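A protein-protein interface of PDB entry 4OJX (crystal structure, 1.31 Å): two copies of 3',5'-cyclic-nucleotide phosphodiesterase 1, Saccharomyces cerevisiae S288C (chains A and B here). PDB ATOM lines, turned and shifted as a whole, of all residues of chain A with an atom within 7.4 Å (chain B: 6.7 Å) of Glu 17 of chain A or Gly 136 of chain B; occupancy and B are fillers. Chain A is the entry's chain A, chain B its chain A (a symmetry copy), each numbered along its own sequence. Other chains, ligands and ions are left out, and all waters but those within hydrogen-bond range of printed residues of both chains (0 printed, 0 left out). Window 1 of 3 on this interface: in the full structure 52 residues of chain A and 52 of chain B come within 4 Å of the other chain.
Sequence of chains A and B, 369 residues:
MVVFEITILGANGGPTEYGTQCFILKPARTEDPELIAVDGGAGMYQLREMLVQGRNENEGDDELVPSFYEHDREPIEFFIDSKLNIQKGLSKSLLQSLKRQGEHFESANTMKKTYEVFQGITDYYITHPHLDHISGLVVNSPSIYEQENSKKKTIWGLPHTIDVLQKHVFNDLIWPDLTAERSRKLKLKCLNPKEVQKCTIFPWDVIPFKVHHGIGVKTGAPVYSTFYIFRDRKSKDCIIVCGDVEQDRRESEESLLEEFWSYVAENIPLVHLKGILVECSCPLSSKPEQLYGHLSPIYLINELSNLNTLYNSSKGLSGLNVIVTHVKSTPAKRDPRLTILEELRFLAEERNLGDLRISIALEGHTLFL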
ATOM      1  N   ASN A  12      -5.235 -10.338   0.634  1.00  0.00           N
ATOM      2  CA  ASN A  12      -4.726 -10.023   1.968  1.00  0.00           C
ATOM      3  C   ASN A  12      -5.520 -10.793   3.017  1.00  0.00           C
ATOM      4  O   ASN A  12      -6.745 -10.731   3.007  1.00  0.00           O
ATOM      5  CB  ASN A  12      -4.880  -8.505   2.147  1.00  0.00           C
ATOM      6  CG  ASN A  12      -4.579  -8.010   3.544  1.00  0.00           C
ATOM      7  OD1 ASN A  12      -3.909  -8.656   4.334  1.00  0.00           O
ATOM      8  ND2 ASN A  12      -5.096  -6.827   3.844  1.00  0.00           N
ATOM      9  N   GLY A  14      -5.412 -10.160   6.259  1.00  0.00           N
ATOM     10  CA  GLY A  14      -5.535  -9.330   7.456  1.00  0.00           C
ATOM     11  C   GLY A  14      -4.235  -9.320   8.239  1.00  0.00           C
ATOM     12  O   GLY A  14      -3.307 -10.068   7.919  1.00  0.00           O
ATOM     13  N   PRO A  15      -4.156  -8.504   9.305  1.00  0.00           N
ATOM     14  CA  PRO A  15      -5.252  -7.727   9.857  1.00  0.00           C
ATOM     15  C   PRO A  15      -5.428  -6.351   9.226  1.00  0.00           C
ATOM     16  O   PRO A  15      -6.385  -5.669   9.569  1.00  0.00           O
ATOM     17  CB  PRO A  15      -4.856  -7.579  11.326  1.00  0.00           C
ATOM     18  CG  PRO A  15      -3.361  -7.508  11.270  1.00  0.00           C
ATOM     19  CD  PRO A  15      -2.983  -8.504  10.204  1.00  0.00           C
ATOM     20  N   THR A  16      -4.550  -5.918   8.320  1.00  0.00           N
ATOM     21  CA  THR A  16      -4.877  -4.682   7.589  1.00  0.00           C
ATOM     22  C   THR A  16      -6.142  -4.942   6.764  1.00  0.00           C
ATOM     23  O   THR A  16      -6.392  -6.071   6.322  1.00  0.00           O
ATOM     24  CB  THR A  16      -3.744  -4.108   6.723  1.00  0.00           C
ATOM     25  OG1 THR A  16      -3.549  -4.933   5.579  1.00  0.00           O
ATOM     26  CG2 THR A  16      -2.452  -3.978   7.507  1.00  0.00           C
ATOM     27  N   GLU A  17      -6.936  -3.901   6.582  1.00  0.00           N
ATOM     28  CA  GLU A  17      -8.344  -4.066   6.251  1.00  0.00           C
ATOM     29  C   GLU A  17      -8.684  -3.900   4.775  1.00  0.00           C
ATOM     30  O   GLU A  17      -9.828  -4.134   4.384  1.00  0.00           O
ATOM     31  CB  GLU A  17      -9.203  -3.130   7.113  1.00  0.00           C
ATOM     32  CG  GLU A  17      -9.165  -1.656   6.718  1.00  0.00           C
ATOM     33  CD  GLU A  17      -7.933  -0.889   7.178  1.00  0.00           C
ATOM     34  OE1 GLU A  17      -7.883   0.324   6.885  1.00  0.00           O
ATOM     35  OE2 GLU A  17      -7.023  -1.469   7.818  1.00  0.00           O
ATOM     36  N   TYR A  18      -7.710  -3.501   3.967  1.00  0.00           N
ATOM     37  CA  TYR A  18      -7.970  -3.324   2.548  1.00  0.00           C
ATOM     38  C   TYR A  18      -7.354  -4.441   1.721  1.00  0.00           C
ATOM     39  O   TYR A  18      -6.361  -5.044   2.100  1.00  0.00           O
ATOM     40  CB  TYR A  18      -7.521  -1.946   2.051  1.00  0.00           C
ATOM     41  CG  TYR A  18      -7.678  -1.779   0.558  1.00  0.00           C
ATOM     42  CD1 TYR A  18      -8.941  -1.788  -0.031  1.00  0.00           C
ATOM     43  CD2 TYR A  18      -6.565  -1.646  -0.267  1.00  0.00           C
ATOM     44  CE1 TYR A  18      -9.090  -1.660  -1.401  1.00  0.00           C
ATOM     45  CE2 TYR A  18      -6.700  -1.507  -1.639  1.00  0.00           C
ATOM     46  CZ  TYR A  18      -7.964  -1.516  -2.197  1.00  0.00           C
ATOM     47  OH  TYR A  18      -8.103  -1.381  -3.556  1.00  0.00           O
ATOM     48  N   GLY A  19      -7.971  -4.706   0.579  1.00  0.00           N
ATOM     49  CA  GLY A  19      -7.484  -5.716  -0.327  1.00  0.00           C
ATOM     50  C   GLY A  19      -7.711  -7.111   0.198  1.00  0.00           C
ATOM     51  O   GLY A  19      -6.951  -8.014  -0.112  1.00  0.00           O
ATOM     52  N   THR A  20      -8.770  -7.297   0.987  1.00  0.00           N
ATOM     53  CA  THR A  20      -9.089  -8.629   1.499  1.00  0.00           C
ATOM     54  C   THR A  20      -9.770  -9.461   0.399  1.00  0.00           C
ATOM     55  O   THR A  20     -10.038  -8.957  -0.698  1.00  0.00           O
ATOM     56  CB  THR A  20      -9.869  -8.571   2.826  1.00  0.00           C
ATOM     57  OG1 THR A  20     -11.067  -7.833   2.648  1.00  0.00           O
ATOM     58  CG2 THR A  20      -9.038  -7.906   3.916  1.00  0.00           C
ATOM     59  N   GLY A  41     -14.383  -9.375  -0.542  1.00  0.00           N
ATOM     60  CA  GLY A  41     -13.544  -8.389   0.141  1.00  0.00           C
ATOM     61  C   GLY A  41     -13.294  -7.216  -0.810  1.00  0.00           C
ATOM     62  O   GLY A  41     -14.215  -6.435  -1.092  1.00  0.00           O
ATOM     63  N   ALA A  42     -12.072  -7.062  -1.314  1.00  0.00           N
ATOM     64  CA  ALA A  42     -11.772  -5.973  -2.259  1.00  0.00           C
ATOM     65  C   ALA A  42     -12.714  -5.987  -3.472  1.00  0.00           C
ATOM     66  O   ALA A  42     -12.897  -7.038  -4.083  1.00  0.00           O
ATOM     67  CB  ALA A  42     -10.323  -6.054  -2.703  1.00  0.00           C
ATOM     68  N   LEU A 131     -16.150 -11.123   7.961  1.00  0.00           N
ATOM     69  CA  LEU A 131     -16.288  -9.786   7.396  1.00  0.00           C
ATOM     70  C   LEU A 131     -15.271  -9.481   6.285  1.00  0.00           C
ATOM     71  O   LEU A 131     -15.613  -8.787   5.330  1.00  0.00           O
ATOM     72  CB  LEU A 131     -16.246  -8.746   8.516  1.00  0.00           C
ATOM     73  CG  LEU A 131     -16.660  -7.315   8.170  1.00  0.00           C
ATOM     74  CD1 LEU A 131     -17.428  -6.693   9.327  1.00  0.00           C
ATOM     75  CD2 LEU A 131     -15.453  -6.476   7.782  1.00  0.00           C
ATOM     76  N   ASP A 132     -14.040  -9.989   6.402  1.00  0.00           N
ATOM     77  CA  ASP A 132     -13.010  -9.754   5.380  1.00  0.00           C
ATOM     78  C   ASP A 132     -13.377 -10.339   4.019  1.00  0.00           C
ATOM     79  O   ASP A 132     -12.787  -9.946   3.006  1.00  0.00           O
ATOM     80  CB  ASP A 132     -11.587 -10.202   5.818  1.00  0.00           C
ATOM     81  CG  ASP A 132     -11.506 -11.683   6.216  1.00  0.00           C
ATOM     82  OD1 ASP A 132     -12.374 -12.074   7.033  1.00  0.00           O
ATOM     83  OD2 ASP A 132     -10.594 -12.464   5.742  1.00  0.00           O
ATOM     84  N   SER A 135     -16.863  -7.529   2.969  1.00  0.00           N
ATOM     85  CA  SER A 135     -16.927  -6.082   3.211  1.00  0.00           C
ATOM     86  C   SER A 135     -17.150  -5.263   1.936  1.00  0.00           C
ATOM     87  O   SER A 135     -17.942  -4.317   1.949  1.00  0.00           O
ATOM     88  CB  SER A 135     -15.672  -5.611   3.942  1.00  0.00           C
ATOM     89  OG  SER A 135     -14.508  -5.971   3.232  1.00  0.00           O
ATOM     90  N   GLU B  17     -15.318   0.894  -1.259  1.00  0.00           N
ATOM     91  CA  GLU B  17     -15.286   0.232   0.037  1.00  0.00           C
ATOM     92  C   GLU B  17     -14.087   0.582   0.911  1.00  0.00           C
ATOM     93  O   GLU B  17     -14.034   0.162   2.067  1.00  0.00           O
ATOM     94  CB  GLU B  17     -15.399  -1.288  -0.143  1.00  0.00           C
ATOM     95  CG  GLU B  17     -14.142  -1.984  -0.656  1.00  0.00           C
ATOM     96  CD  GLU B  17     -13.895  -1.862  -2.154  1.00  0.00           C
ATOM     97  OE1 GLU B  17     -12.883  -2.437  -2.606  1.00  0.00           O
ATOM     98  OE2 GLU B  17     -14.683  -1.209  -2.879  1.00  0.00           O
ATOM     99  N   TYR B  18     -13.140   1.338   0.370  1.00  0.00           N
ATOM    100  CA  TYR B  18     -11.971   1.707   1.153  1.00  0.00           C
ATOM    101  C   TYR B  18     -12.020   3.164   1.582  1.00  0.00           C
ATOM    102  O   TYR B  18     -12.620   4.004   0.927  1.00  0.00           O
ATOM    103  CB  TYR B  18     -10.666   1.382   0.419  1.00  0.00           C
ATOM    104  CG  TYR B  18      -9.439   1.857   1.161  1.00  0.00           C
ATOM    105  CD1 TYR B  18      -9.100   1.313   2.398  1.00  0.00           C
ATOM    106  CD2 TYR B  18      -8.640   2.874   0.645  1.00  0.00           C
ATOM    107  CE1 TYR B  18      -7.991   1.761   3.094  1.00  0.00           C
ATOM    108  CE2 TYR B  18      -7.522   3.325   1.327  1.00  0.00           C
ATOM    109  CZ  TYR B  18      -7.206   2.765   2.549  1.00  0.00           C
ATOM    110  OH  TYR B  18      -6.100   3.210   3.230  1.00  0.00           O
ATOM    111  N   GLY B  19     -11.376   3.445   2.704  1.00  0.00           N
ATOM    112  CA  GLY B  19     -11.307   4.790   3.220  1.00  0.00           C
ATOM    113  C   GLY B  19     -12.627   5.255   3.780  1.00  0.00           C
ATOM    114  O   GLY B  19     -12.917   6.440   3.761  1.00  0.00           O
ATOM    115  N   THR B  20     -13.429   4.323   4.296  1.00  0.00           N
ATOM    116  CA  THR B  20     -14.705   4.697   4.904  1.00  0.00           C
ATOM    117  C   THR B  20     -14.466   5.263   6.314  1.00  0.00           C
ATOM    118  O   THR B  20     -13.330   5.282   6.802  1.00  0.00           O
ATOM    119  CB  THR B  20     -15.735   3.552   4.847  1.00  0.00           C
ATOM    120  OG1 THR B  20     -15.216   2.406   5.501  1.00  0.00           O
ATOM    121  CG2 THR B  20     -16.062   3.189   3.403  1.00  0.00           C
ATOM    122  N   GLY B  40     -14.800   3.427  12.776  1.00  0.00           N
ATOM    123  CA  GLY B  40     -13.882   2.318  12.593  1.00  0.00           C
ATOM    124  C   GLY B  40     -13.913   1.763  11.195  1.00  0.00           C
ATOM    125  O   GLY B  40     -13.773   0.550  11.002  1.00  0.00           O
ATOM    126  N   GLY B  41     -14.063   2.648  10.209  1.00  0.00           N
ATOM    127  CA  GLY B  41     -13.874   2.280   8.805  1.00  0.00           C
ATOM    128  C   GLY B  41     -12.374   2.158   8.528  1.00  0.00           C
ATOM    129  O   GLY B  41     -11.727   1.212   9.002  1.00  0.00           O
ATOM    130  N   ALA B  42     -11.796   3.086   7.769  1.00  0.00           N
ATOM    131  CA  ALA B  42     -10.350   3.045   7.489  1.00  0.00           C
ATOM    132  C   ALA B  42      -9.516   2.995   8.778  1.00  0.00           C
ATOM    133  O   ALA B  42      -9.749   3.796   9.681  1.00  0.00           O
ATOM    134  CB  ALA B  42      -9.952   4.236   6.637  1.00  0.00           C
ATOM    135  N   GLY B  43      -8.529   2.084   8.835  1.00  0.00           N
ATOM    136  CA  GLY B  43      -7.728   1.829  10.044  1.00  0.00           C
ATOM    137  C   GLY B  43      -6.244   1.593   9.772  1.00  0.00           C
ATOM    138  O   GLY B  43      -5.567   2.468   9.208  1.00  0.00           O
ATOM    139  N   MET B  44      -5.735   0.421  10.170  1.00  0.00           N
ATOM    140  CA  MET B  44      -4.312   0.100   9.978  1.00  0.00           C
ATOM    141  C   MET B  44      -3.792   0.345   8.575  1.00  0.00           C
ATOM    142  O   MET B  44      -2.683   0.852   8.408  1.00  0.00           O
ATOM    143  CB  MET B  44      -4.049  -1.373  10.272  1.00  0.00           C
ATOM    144  CG  MET B  44      -4.051  -1.743  11.723  1.00  0.00           C
ATOM    145  SD  MET B  44      -3.639  -3.482  11.895  1.00  0.00           S
ATOM    146  CE  MET B  44      -1.861  -3.436  11.909  1.00  0.00           C
ATOM    147  N   TYR B  45      -4.553  -0.081   7.569  1.00  0.00           N
ATOM    148  CA  TYR B  45      -4.097   0.052   6.194  1.00  0.00           C
ATOM    149  C   TYR B  45      -3.826   1.523   5.875  1.00  0.00           C
ATOM    150  O   TYR B  45      -2.837   1.864   5.215  1.00  0.00           O
ATOM    151  CB  TYR B  45      -5.143  -0.529   5.237  1.00  0.00           C
ATOM    152  CG  TYR B  45      -4.686  -0.672   3.807  1.00  0.00           C
ATOM    153  CD1 TYR B  45      -4.672   0.426   2.948  1.00  0.00           C
ATOM    154  CD2 TYR B  45      -4.286  -1.910   3.305  1.00  0.00           C
ATOM    155  CE1 TYR B  45      -4.264   0.299   1.630  1.00  0.00           C
ATOM    156  CE2 TYR B  45      -3.878  -2.049   1.991  1.00  0.00           C
ATOM    157  CZ  TYR B  45      -3.863  -0.940   1.163  1.00  0.00           C
ATOM    158  OH  TYR B  45      -3.456  -1.074  -0.145  1.00  0.00           O
ATOM    159  N   GLN B  46      -4.705   2.398   6.347  1.00  0.00           N
ATOM    160  CA  GLN B  46      -4.558   3.808   6.056  1.00  0.00           C
ATOM    161  C   GLN B  46      -3.419   4.451   6.847  1.00  0.00           C
ATOM    162  O   GLN B  46      -2.700   5.303   6.323  1.00  0.00           O
ATOM    163  CB  GLN B  46      -5.879   4.550   6.260  1.00  0.00           C
ATOM    164  CG  GLN B  46      -5.859   6.014   5.831  1.00  0.00           C
ATOM    165  CD  GLN B  46      -5.264   6.267   4.450  1.00  0.00           C
ATOM    166  OE1 GLN B  46      -5.480   5.507   3.504  1.00  0.00           O
ATOM    167  NE2 GLN B  46      -4.504   7.352   4.334  1.00  0.00           N
ATOM    168  N   LEU B  47      -3.245   4.035   8.097  1.00  0.00           N
ATOM    169  CA  LEU B  47      -2.097   4.481   8.875  1.00  0.00           C
ATOM    170  C   LEU B  47      -0.794   4.131   8.153  1.00  0.00           C
ATOM    171  O   LEU B  47       0.122   4.951   8.078  1.00  0.00           O
ATOM    172  CB  LEU B  47      -2.119   3.866  10.273  1.00  0.00           C
ATOM    173  CG  LEU B  47      -3.169   4.445  11.220  1.00  0.00           C
ATOM    174  CD1 LEU B  47      -3.277   3.587  12.466  1.00  0.00           C
ATOM    175  CD2 LEU B  47      -2.820   5.884  11.591  1.00  0.00           C
ATOM    176  N   PHE B 118      -0.582   1.692  15.667  1.00  0.00           N
ATOM    177  CA  PHE B 118      -1.922   1.206  15.837  1.00  0.00           C
ATOM    178  C   PHE B 118      -2.197   0.652  17.240  1.00  0.00           C
ATOM    179  O   PHE B 118      -3.319   0.728  17.732  1.00  0.00           O
ATOM    180  CB  PHE B 118      -2.237   0.176  14.763  1.00  0.00           C
ATOM    181  CG  PHE B 118      -3.662  -0.220  14.740  1.00  0.00           C
ATOM    182  CD1 PHE B 118      -4.656   0.707  14.430  1.00  0.00           C
ATOM    183  CD2 PHE B 118      -4.021  -1.510  15.078  1.00  0.00           C
ATOM    184  CE1 PHE B 118      -5.993   0.337  14.431  1.00  0.00           C
ATOM    185  CE2 PHE B 118      -5.356  -1.890  15.071  1.00  0.00           C
ATOM    186  CZ  PHE B 118      -6.343  -0.963  14.753  1.00  0.00           C
ATOM    187  N   TYR B 124     -12.319   3.285  20.742  1.00  0.00           N
ATOM    188  CA  TYR B 124     -13.139   3.669  19.590  1.00  0.00           C
ATOM    189  C   TYR B 124     -14.476   4.170  20.101  1.00  0.00           C
ATOM    190  O   TYR B 124     -15.064   3.560  21.001  1.00  0.00           O
ATOM    191  CB  TYR B 124     -13.437   2.473  18.695  1.00  0.00           C
ATOM    192  CG  TYR B 124     -12.287   1.844  17.968  1.00  0.00           C
ATOM    193  CD1 TYR B 124     -11.409   0.981  18.616  1.00  0.00           C
ATOM    194  CD2 TYR B 124     -12.114   2.065  16.610  1.00  0.00           C
ATOM    195  CE1 TYR B 124     -10.370   0.379  17.921  1.00  0.00           C
ATOM    196  CE2 TYR B 124     -11.084   1.473  15.904  1.00  0.00           C
ATOM    197  CZ  TYR B 124     -10.214   0.634  16.564  1.00  0.00           C
ATOM    198  OH  TYR B 124      -9.204   0.013  15.859  1.00  0.00           O
ATOM    199  N   LEU B 131     -21.775  -1.298   8.356  1.00  0.00           N
ATOM    200  CA  LEU B 131     -20.491  -1.946   8.117  1.00  0.00           C
ATOM    201  C   LEU B 131     -19.372  -0.968   7.730  1.00  0.00           C
ATOM    202  O   LEU B 131     -18.225  -1.179   8.121  1.00  0.00           O
ATOM    203  CB  LEU B 131     -20.662  -3.063   7.087  1.00  0.00           C
ATOM    204  CG  LEU B 131     -19.505  -4.048   6.912  1.00  0.00           C
ATOM    205  CD1 LEU B 131     -20.038  -5.453   6.669  1.00  0.00           C
ATOM    206  CD2 LEU B 131     -18.571  -3.602   5.799  1.00  0.00           C
ATOM    207  N   ASP B 132     -19.692   0.087   6.973  1.00  0.00           N
ATOM    208  CA  ASP B 132     -18.684   1.076   6.566  1.00  0.00           C
ATOM    209  C   ASP B 132     -18.062   1.814   7.748  1.00  0.00           C
ATOM    210  O   ASP B 132     -16.994   2.418   7.597  1.00  0.00           O
ATOM    211  CB  ASP B 132     -19.193   2.073   5.487  1.00  0.00           C
ATOM    212  CG  ASP B 132     -20.449   2.849   5.913  1.00  0.00           C
ATOM    213  OD1 ASP B 132     -21.390   2.153   6.365  1.00  0.00           O
ATOM    214  OD2 ASP B 132     -20.524   4.133   5.799  1.00  0.00           O
ATOM    215  N   HIS B 133     -18.706   1.762   8.919  1.00  0.00           N
ATOM    216  CA  HIS B 133     -18.198   2.439  10.115  1.00  0.00           C
ATOM    217  C   HIS B 133     -17.497   1.519  11.062  1.00  0.00           C
ATOM    218  O   HIS B 133     -17.012   1.979  12.092  1.00  0.00           O
ATOM    219  CB  HIS B 133     -19.321   3.213  10.820  1.00  0.00           C
ATOM    220  CG  HIS B 133     -19.896   4.289   9.956  1.00  0.00           C
ATOM    221  ND1 HIS B 133     -19.663   5.613  10.140  1.00  0.00           N
ATOM    222  CD2 HIS B 133     -20.650   4.184   8.813  1.00  0.00           C
ATOM    223  CE1 HIS B 133     -20.248   6.302   9.148  1.00  0.00           C
ATOM    224  NE2 HIS B 133     -20.843   5.429   8.339  1.00  0.00           N
ATOM    225  N   ILE B 134     -17.400   0.235  10.713  1.00  0.00           N
ATOM    226  CA  ILE B 134     -16.777  -0.734  11.612  1.00  0.00           C
ATOM    227  C   ILE B 134     -15.831  -1.719  10.925  1.00  0.00           C
ATOM    228  O   ILE B 134     -15.206  -2.511  11.609  1.00  0.00           O
ATOM    229  CB  ILE B 134     -17.823  -1.537  12.422  1.00  0.00           C
ATOM    230  CG1 ILE B 134     -18.720  -2.357  11.484  1.00  0.00           C
ATOM    231  CG2 ILE B 134     -18.613  -0.609  13.338  1.00  0.00           C
ATOM    232  CD1 ILE B 134     -19.553  -3.421  12.170  1.00  0.00           C
ATOM    233  N   SER B 135     -15.721  -1.683   9.601  1.00  0.00           N
ATOM    234  CA  SER B 135     -14.971  -2.718   8.878  1.00  0.00           C
ATOM    235  C   SER B 135     -13.493  -2.783   9.272  1.00  0.00           C
ATOM    236  O   SER B 135     -12.952  -3.880   9.435  1.00  0.00           O
ATOM    237  CB  SER B 135     -15.120  -2.525   7.371  1.00  0.00           C
ATOM    238  OG  SER B 135     -14.724  -1.227   6.986  1.00  0.00           O
ATOM    239  N   GLY B 136     -12.845  -1.628   9.442  1.00  0.00           N
ATOM    240  CA  GLY B 136     -11.445  -1.613   9.864  1.00  0.00           C
ATOM    241  C   GLY B 136     -11.277  -2.020  11.310  1.00  0.00           C
ATOM    242  O   GLY B 136     -10.397  -2.813  11.640  1.00  0.00           O
ATOM    243  N   LEU B 137     -12.125  -1.496  12.186  1.00  0.00           N
ATOM    244  CA  LEU B 137     -12.132  -1.933  13.570  1.00  0.00           C
ATOM    245  C   LEU B 137     -12.156  -3.464  13.642  1.00  0.00           C
ATOM    246  O   LEU B 137     -11.380  -4.080  14.382  1.00  0.00           O
ATOM    247  CB  LEU B 137     -13.358  -1.360  14.287  1.00  0.00           C
ATOM    248  CG  LEU B 137     -13.817  -2.044  15.582  1.00  0.00           C
ATOM    249  CD1 LEU B 137     -12.776  -1.911  16.687  1.00  0.00           C
ATOM    250  CD2 LEU B 137     -15.176  -1.508  16.017  1.00  0.00           C
ATOM    251  N   VAL B 138     -13.054  -4.078  12.879  1.00  0.00           N
ATOM    252  CA  VAL B 138     -13.227  -5.517  12.936  1.00  0.00           C
ATOM    253  C   VAL B 138     -12.016  -6.249  12.359  1.00  0.00           C
ATOM    254  O   VAL B 138     -11.409  -7.083  13.024  1.00  0.00           O
ATOM    255  CB  VAL B 138     -14.535  -5.941  12.243  1.00  0.00           C
ATOM    256  CG1 VAL B 138     -14.612  -7.457  12.126  1.00  0.00           C
ATOM    257  CG2 VAL B 138     -15.735  -5.398  13.013  1.00  0.00           C
ATOM    258  N   VAL B 139     -11.654  -5.939  11.124  1.00  0.00           N
ATOM    259  CA  VAL B 139     -10.580  -6.696  10.479  1.00  0.00           C
ATOM    260  C   VAL B 139      -9.236  -6.464  11.186  1.00  0.00           C
ATOM    261  O   VAL B 139      -8.423  -7.382  11.291  1.00  0.00           O
ATOM    262  CB  VAL B 139     -10.525  -6.452   8.964  1.00  0.00           C
ATOM    263  CG1 VAL B 139      -9.378  -7.228   8.336  1.00  0.00           C
ATOM    264  CG2 VAL B 139     -11.852  -6.863   8.328  1.00  0.00           C
ATOM    265  N   ASN B 140      -9.028  -5.255  11.716  1.00  0.00           N
ATOM    266  CA  ASN B 140      -7.782  -4.932  12.418  1.00  0.00           C
ATOM    267  C   ASN B 140      -7.694  -5.596  13.793  1.00  0.00           C
ATOM    268  O   ASN B 140      -6.602  -5.731  14.342  1.00  0.00           O
ATOM    269  CB  ASN B 140      -7.623  -3.423  12.679  1.00  0.00           C
ATOM    270  CG  ASN B 140      -7.500  -2.552  11.430  1.00  0.00           C
ATOM    271  OD1 ASN B 140      -7.582  -1.327  11.566  1.00  0.00           O
ATOM    272  ND2 ASN B 140      -7.275  -3.127  10.252  1.00  0.00           N
ATOM    273  N   SER B 141      -8.833  -5.981  14.363  1.00  0.00           N
ATOM    274  CA  SER B 141      -8.876  -6.373  15.778  1.00  0.00           C
ATOM    275  C   SER B 141      -7.917  -7.495  16.213  1.00  0.00           C
ATOM    276  O   SER B 141      -7.422  -7.441  17.326  1.00  0.00           O
ATOM    277  CB  SER B 141     -10.322  -6.628  16.256  1.00  0.00           C
ATOM    278  OG  SER B 141     -10.937  -7.713  15.579  1.00  0.00           O
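The backbone carbonyl oxygen of Pro 15 of chain A sits at hydrogen-bond distance from the side-chain amide nitrogen of Asn 140 of chain B, 2.8 Å away. N of Gly 43 of chain B sits at hydrogen-bond distance from OE1 of Glu 17 of chain A, 2.7 Å away. The side-chain carboxylate (OE2) of Glu 17 of chain A is in hydrogen-bond range of the backbone NH (N) of Met 44 of chain B, at 3.3 Å. N of Tyr 45 of chain B sits at hydrogen-bond distance from OE2 of Glu 17 of chain A (2.8 Å). ND2 of Asn 140 of chain B is in hydrogen-bond range of OE2 of Glu 17 of chain A, at 3.0 Å. O of Pro 15 of chain A sits close to O of Val 139 of chain B, 3.2 Å away.
The side-chain amide nitrogen (ND2) of Asn 12 of chain A is in hydrogen-bond range of the backbone carbonyl oxygen (O) of Thr 16 of chain A, at 2.9 Å. The backbone NH of Ala 42 of chain A lies within hydrogen-bond range of the backbone carbonyl oxygen of Thr 20 of chain A (2.8 Å). The backbone NH of Ala 42 of chain B is in hydrogen-bond range of the backbone carbonyl oxygen of Thr 20 of chain B, at 2.8 Å. The backbone carbonyl oxygen (O) of Gly 40 of chain B lies within hydrogen-bond range of the backbone NH (N) of Gly 136 of chain B, 2.8 Å away. The backbone NH (N) of Met 44 of chain B is in hydrogen-bond range of the side-chain amide oxygen (OD1) of Asn 140 of chain B (2.9 Å). The backbone carbonyl oxygen of Gly 136 of chain B sits close to the side-chain amide oxygen of Asn 140 of chain B, 3.2 Å away.
Among the printed residues, merely in contact across the chains: Thr 16 of chain A with Tyr 45 of chain B (3.9 Å), Thr 16 of chain A with Val 139 of chain B (3.8 Å), Thr 16 of chain A with Asn 140 of chain B (3.9 Å), Glu 17 of chain A with Ala 42 of chain B (3.7 Å), Glu 17 of chain A with Gln 46 of chain B (3.8 Å), Glu 17 of chain A with Gly 136 of chain B (3.9 Å), Glu 17 of chain A with Val 139 of chain B (3.9 Å), Tyr 18 of chain A with Tyr 18 of chain B (3.6 Å), Tyr 18 of chain A with Tyr 45 of chain B (3.1 Å), Ala 42 of chain A with Glu 17 of chain B (3.7 Å), Leu 131 of chain A with Leu 131 of chain B (3.9 Å), Leu 131 of chain A with Ser 135 of chain B (3.9 Å), Leu 131 of chain A with Val 139 of chain B (3.7 Å) and Ser 135 of chain A with Leu 131 of chain B (3.9 Å).
Glu 17 of chain A touches just these residues of chain B: Ala 42, Gly 43, Met 44, Tyr 45, Gln 46, Gly 136, Val 139 and Asn 140. Gly 136 of chain B touches one residue of chain A. Ser 135 of chain B touches just one residue of chain A: Leu 131. Of the printed residues of chain A, Leu 131 of chain B touches Leu 131 and Ser 135. Of the printed residues of chain A, Gly 43 of chain B touches Glu 17. The nearest residue of chain B that does not touch Glu 17 of chain A is Tyr 18 of chain B (4.1 Å).
Of the 25 printed residues of chain B, 12 touch a printed residue of chain A. Hydrophobic or aromatic side chains of chain B within 4 Å of the printed part of chain A: Tyr 18, Met 44, Tyr 45, Leu 131 and Val 139. Among the printed residues, no Asp or Glu carboxylate lies within 4 Å of a Lys or Arg side-chain nitrogen of the other chain.
Glu 17 of chain A touches Ala 42 of chain B, and with the chains exchanged Ala 42 of chain A touches Glu 17 of chain B. Tyr 18 of chain B touches its own counterpart, Tyr 18 of chain A. Leu 131 of chain B touches its own counterpart, Leu 131 of chain A. Leu 131 of chain A touches Ser 135 of chain B, and with the chains exchanged Ser 135 of chain A touches Leu 131 of chain B. Positions printed for both chains: 17, 18, 19, 20, 41, 42, 131, 132 and 135. Of the 20 pairs that touch across the chains among the printed residues, 6 have their exchanged pair printed and touching as well.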
